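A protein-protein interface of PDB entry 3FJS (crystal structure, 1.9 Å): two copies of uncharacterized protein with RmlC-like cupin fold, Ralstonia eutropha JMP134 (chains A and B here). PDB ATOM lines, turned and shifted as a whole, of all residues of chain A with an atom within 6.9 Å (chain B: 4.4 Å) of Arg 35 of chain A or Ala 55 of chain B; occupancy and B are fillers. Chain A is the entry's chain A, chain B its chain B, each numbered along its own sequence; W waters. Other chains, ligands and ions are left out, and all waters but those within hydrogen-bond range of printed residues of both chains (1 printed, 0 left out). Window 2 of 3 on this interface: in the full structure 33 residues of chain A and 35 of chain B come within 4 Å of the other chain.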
ATOM      1  N   LYS A  32      31.081 -30.654  -5.091  1.00  0.00           N
ATOM      2  CA  LYS A  32      31.231 -29.280  -5.418  1.00  0.00           C
ATOM      3  C   LYS A  32      29.831 -28.799  -5.763  1.00  0.00           C
ATOM      4  O   LYS A  32      29.208 -29.332  -6.673  1.00  0.00           O
ATOM      5  CB  LYS A  32      32.232 -29.169  -6.580  1.00  0.00           C
ATOM      6  CG  LYS A  32      32.295 -27.842  -7.276  1.00  0.00           C
ATOM      7  CD  LYS A  32      32.896 -26.767  -6.426  1.00  0.00           C
ATOM      8  CE  LYS A  32      32.536 -25.386  -6.927  1.00  0.00           C
ATOM      9  NZ  LYS A  32      31.116 -25.130  -6.621  1.00  0.00           N
ATOM     10  N   GLU A  33      29.323 -27.847  -4.993  1.00  0.00           N
ATOM     11  CA  GLU A  33      28.014 -27.272  -5.241  1.00  0.00           C
ATOM     12  C   GLU A  33      28.139 -25.752  -5.162  1.00  0.00           C
ATOM     13  O   GLU A  33      29.205 -25.226  -4.814  1.00  0.00           O
ATOM     14  CB  GLU A  33      26.948 -27.839  -4.287  1.00  0.00           C
ATOM     15  CG  GLU A  33      27.112 -27.400  -2.828  1.00  0.00           C
ATOM     16  CD  GLU A  33      25.825 -26.864  -2.274  1.00  0.00           C
ATOM     17  OE1 GLU A  33      25.011 -27.677  -1.805  1.00  0.00           O
ATOM     18  OE2 GLU A  33      25.659 -25.618  -2.297  1.00  0.00           O
ATOM     19  N   HIS A  34      27.042 -25.068  -5.471  1.00  0.00           N
ATOM     20  CA  HIS A  34      27.020 -23.609  -5.511  1.00  0.00           C
ATOM     21  C   HIS A  34      27.612 -22.874  -4.263  1.00  0.00           C
ATOM     22  O   HIS A  34      28.381 -21.934  -4.417  1.00  0.00           O
ATOM     23  CB  HIS A  34      25.599 -23.153  -5.816  1.00  0.00           C
ATOM     24  CG  HIS A  34      25.433 -21.674  -5.881  1.00  0.00           C
ATOM     25  ND1 HIS A  34      26.100 -20.891  -6.800  1.00  0.00           N
ATOM     26  CD2 HIS A  34      24.648 -20.838  -5.167  1.00  0.00           C
ATOM     27  CE1 HIS A  34      25.741 -19.631  -6.639  1.00  0.00           C
ATOM     28  NE2 HIS A  34      24.864 -19.571  -5.652  1.00  0.00           N
ATOM     29  N   ARG A  35      27.280 -23.324  -3.057  1.00  0.00           N
ATOM     30  CA  ARG A  35      27.753 -22.666  -1.829  1.00  0.00           C
ATOM     31  C   ARG A  35      28.810 -23.426  -1.021  1.00  0.00           C
ATOM     32  O   ARG A  35      29.240 -22.923   0.016  1.00  0.00           O
ATOM     33  CB  ARG A  35      26.561 -22.413  -0.900  1.00  0.00           C
ATOM     34  CG  ARG A  35      25.407 -21.638  -1.490  1.00  0.00           C
ATOM     35  CD  ARG A  35      24.478 -21.223  -0.372  1.00  0.00           C
ATOM     36  NE  ARG A  35      23.315 -20.483  -0.862  1.00  0.00           N
ATOM     37  CZ  ARG A  35      22.048 -20.905  -0.883  1.00  0.00           C
ATOM     38  NH1 ARG A  35      21.665 -22.101  -0.382  1.00  0.00           N
ATOM     39  NH2 ARG A  35      21.120 -20.080  -1.386  1.00  0.00           N
ATOM     40  N   LEU A  36      29.274 -24.575  -1.497  1.00  0.00           N
ATOM     41  CA  LEU A  36      30.151 -25.439  -0.688  1.00  0.00           C
ATOM     42  C   LEU A  36      30.934 -26.418  -1.541  1.00  0.00           C
ATOM     43  O   LEU A  36      30.387 -26.989  -2.470  1.00  0.00           O
ATOM     44  CB  LEU A  36      29.271 -26.230   0.312  1.00  0.00           C
ATOM     45  CG  LEU A  36      29.889 -27.173   1.365  1.00  0.00           C
ATOM     46  CD1 LEU A  36      30.728 -26.389   2.372  1.00  0.00           C
ATOM     47  CD2 LEU A  36      28.755 -27.921   2.113  1.00  0.00           C
ATOM     48  N   GLU A  37      32.209 -26.601  -1.200  1.00  0.00           N
ATOM     49  CA  GLU A  37      33.053 -27.600  -1.811  1.00  0.00           C
ATOM     50  C   GLU A  37      33.745 -28.403  -0.684  1.00  0.00           C
ATOM     51  O   GLU A  37      34.212 -27.803   0.282  1.00  0.00           O
ATOM     52  CB  GLU A  37      34.054 -26.913  -2.707  1.00  0.00           C
ATOM     53  CG  GLU A  37      34.979 -27.822  -3.474  1.00  0.00           C
ATOM     54  CD  GLU A  37      35.751 -27.074  -4.591  1.00  0.00           C
ATOM     55  OE1 GLU A  37      35.613 -25.821  -4.719  1.00  0.00           O
ATOM     56  OE2 GLU A  37      36.468 -27.770  -5.356  1.00  0.00           O
ATOM     57  N   VAL A 106      35.069 -25.910   2.160  1.00  0.00           N
ATOM     58  CA  VAL A 106      35.191 -24.517   1.806  1.00  0.00           C
ATOM     59  C   VAL A 106      33.858 -23.909   1.495  1.00  0.00           C
ATOM     60  O   VAL A 106      33.131 -24.418   0.644  1.00  0.00           O
ATOM     61  CB  VAL A 106      36.177 -24.337   0.607  1.00  0.00           C
ATOM     62  CG1 VAL A 106      36.353 -22.827   0.294  1.00  0.00           C
ATOM     63  CG2 VAL A 106      37.488 -24.961   0.931  1.00  0.00           C
ATOM     64  N   VAL A 107      33.512 -22.843   2.210  1.00  0.00           N
ATOM     65  CA  VAL A 107      32.285 -22.107   1.937  1.00  0.00           C
ATOM     66  C   VAL A 107      32.587 -21.219   0.710  1.00  0.00           C
ATOM     67  O   VAL A 107      33.601 -20.535   0.685  1.00  0.00           O
ATOM     68  CB  VAL A 107      31.837 -21.280   3.143  1.00  0.00           C
ATOM     69  CG1 VAL A 107      30.589 -20.429   2.803  1.00  0.00           C
ATOM     70  CG2 VAL A 107      31.582 -22.180   4.306  1.00  0.00           C
ATOM     71  N   LEU A 108      31.718 -21.268  -0.299  1.00  0.00           N
ATOM     72  CA  LEU A 108      31.885 -20.536  -1.540  1.00  0.00           C
ATOM     73  C   LEU A 108      30.988 -19.299  -1.521  1.00  0.00           C
ATOM     74  O   LEU A 108      29.787 -19.420  -1.297  1.00  0.00           O
ATOM     75  CB  LEU A 108      31.551 -21.436  -2.743  1.00  0.00           C
ATOM     76  CG  LEU A 108      32.348 -22.752  -2.888  1.00  0.00           C
ATOM     77  CD1 LEU A 108      31.936 -23.536  -4.119  1.00  0.00           C
ATOM     78  CD2 LEU A 108      33.868 -22.538  -2.903  1.00  0.00           C
ATOM     79  N   VAL A 109      31.578 -18.122  -1.764  1.00  0.00           N
ATOM     80  CA  VAL A 109      30.847 -16.844  -1.737  1.00  0.00           C
ATOM     81  C   VAL A 109      30.660 -16.264  -3.141  1.00  0.00           C
ATOM     82  O   VAL A 109      31.492 -16.475  -4.033  1.00  0.00           O
ATOM     83  CB  VAL A 109      31.535 -15.804  -0.792  1.00  0.00           C
ATOM     84  CG1 VAL A 109      31.630 -16.355   0.623  1.00  0.00           C
ATOM     85  CG2 VAL A 109      32.884 -15.396  -1.286  1.00  0.00           C
ATOM     86  N   VAL B  54      17.743 -27.385   7.274  1.00  0.00           N
ATOM     87  CA  VAL B  54      18.406 -26.091   7.419  1.00  0.00           C
ATOM     88  C   VAL B  54      18.486 -25.470   6.011  1.00  0.00           C
ATOM     89  O   VAL B  54      18.482 -26.186   4.981  1.00  0.00           O
ATOM     90  CB  VAL B  54      19.761 -26.193   8.139  1.00  0.00           C
ATOM     91  CG1 VAL B  54      19.493 -26.605   9.599  1.00  0.00           C
ATOM     92  CG2 VAL B  54      20.738 -27.170   7.410  1.00  0.00           C
ATOM     93  N   ALA B  55      18.519 -24.140   5.973  1.00  0.00           N
ATOM     94  CA  ALA B  55      18.472 -23.411   4.721  1.00  0.00           C
ATOM     95  C   ALA B  55      19.719 -23.576   3.877  1.00  0.00           C
ATOM     96  O   ALA B  55      19.627 -23.463   2.681  1.00  0.00           O
ATOM     97  CB  ALA B  55      18.183 -21.932   4.955  1.00  0.00           C
ATOM     98  N   GLY B  56      20.888 -23.790   4.483  1.00  0.00           N
ATOM     99  CA  GLY B  56      22.097 -23.983   3.697  1.00  0.00           C
ATOM    100  C   GLY B  56      22.487 -25.438   3.582  1.00  0.00           C
ATOM    101  O   GLY B  56      21.902 -26.324   4.262  1.00  0.00           O
ATOM    102  N   PRO B  57      23.511 -25.714   2.729  1.00  0.00           N
ATOM    103  CA  PRO B  57      23.963 -27.080   2.648  1.00  0.00           C
ATOM    104  C   PRO B  57      24.723 -27.447   3.914  1.00  0.00           C
ATOM    105  O   PRO B  57      25.149 -26.567   4.665  1.00  0.00           O
ATOM    106  CB  PRO B  57      24.894 -27.077   1.436  1.00  0.00           C
ATOM    107  CG  PRO B  57      25.467 -25.695   1.414  1.00  0.00           C
ATOM    108  CD  PRO B  57      24.269 -24.824   1.806  1.00  0.00           C
ATOM    109  N   ALA B  88      20.969 -27.891   0.520  1.00  0.00           N
ATOM    110  CA  ALA B  88      20.179 -26.844   1.180  1.00  0.00           C
ATOM    111  C   ALA B  88      18.726 -27.252   1.264  1.00  0.00           C
ATOM    112  O   ALA B  88      18.137 -27.609   0.253  1.00  0.00           O
ATOM    113  CB  ALA B  88      20.288 -25.534   0.428  1.00  0.00           C
ATOM    114  N   GLY B  89      18.169 -27.230   2.470  1.00  0.00           N
ATOM    115  CA  GLY B  89      16.785 -27.589   2.692  1.00  0.00           C
ATOM    116  C   GLY B  89      16.445 -29.073   2.642  1.00  0.00           C
ATOM    117  O   GLY B  89      15.260 -29.412   2.709  1.00  0.00           O
ATOM    118  N   VAL B 107      26.472 -24.611   6.491  1.00  0.00           N
ATOM    119  CA  VAL B 107      26.687 -23.366   5.777  1.00  0.00           C
ATOM    120  C   VAL B 107      25.453 -22.512   6.096  1.00  0.00           C
ATOM    121  O   VAL B 107      24.326 -22.989   6.025  1.00  0.00           O
ATOM    122  CB  VAL B 107      26.834 -23.575   4.255  1.00  0.00           C
ATOM    123  CG1 VAL B 107      26.882 -22.222   3.498  1.00  0.00           C
ATOM    124  CG2 VAL B 107      28.039 -24.470   3.945  1.00  0.00           C
ATOM    125  N   VAL B 109      23.177 -19.175   5.221  1.00  0.00           N
ATOM    126  CA  VAL B 109      22.863 -18.262   4.136  1.00  0.00           C
ATOM    127  C   VAL B 109      22.072 -17.079   4.713  1.00  0.00           C
ATOM    128  O   VAL B 109      21.465 -16.337   3.963  1.00  0.00           O
ATOM    129  CB  VAL B 109      22.100 -18.983   2.984  1.00  0.00           C
ATOM    130  CG1 VAL B 109      22.913 -20.200   2.513  1.00  0.00           C
ATOM    131  CG2 VAL B 109      20.706 -19.406   3.410  1.00  0.00           C
HETATM  132  O   HOH W   1      22.463 -27.213  -1.693  1.00  0.00           O
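O of Arg 35 of chain A lies within hydrogen-bond range of N of Leu 108 of chain A. N of Arg 35 of chain A is in hydrogen-bond range of OE2 of Glu 33 of chain A (2.9 Å). N of Val 107 of chain B lies within hydrogen-bond range of O of Pro 57 of chain B (3.0 Å).
Pro 57 of chain B touches Glu 33 of chain A. Arg 35 of chain A touches Ala 55 of chain B. Arg 35 of chain A touches Ala 88 of chain B (NH1 to CB, 3.8 Å). Arg 35 of chain A touches Val 109 of chain B (NE to CG1, 3.4 Å). Leu 36 of chain A touches Pro 57 of chain B (CB to CG, 3.996 Å). Val 107 of chain B touches Leu 36 of chain A (CG2 to CD1, 3.7 Å).
Of the printed residues of chain B, Glu 33 of chain A touches Pro 57. Of chain B, only Ala 55, Ala 88 and Val 109 come within 4 Å of Arg 35 of chain A. Printed residues of chain B within 4 Å of Leu 36 of chain A: Pro 57 and Val 107. Val 106 of chain A touches none of the printed residues of chain B. Gly 56 of chain B touches none of the printed residues of chain A. Of the printed residues of chain A, Pro 57 of chain B touches Glu 33 and Leu 36. Printed residues of chain A within 4 Å of Val 107 of chain B: Leu 36. Of the printed residues of chain A, Val 109 of chain B touches Arg 35 (3.4 Å).
Among the printed residues, 6 pairs touch across the chains. Among the printed residues, no Asp or Glu carboxylate lies within 4 Å of a Lys or Arg side-chain nitrogen of the other chain.
Positions printed for both chains: 107 and 109.
Water W1 bridges OE1 of Glu 33 of chain A (2.6 Å) and N of Ala 88 of chain B (2.8 Å).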
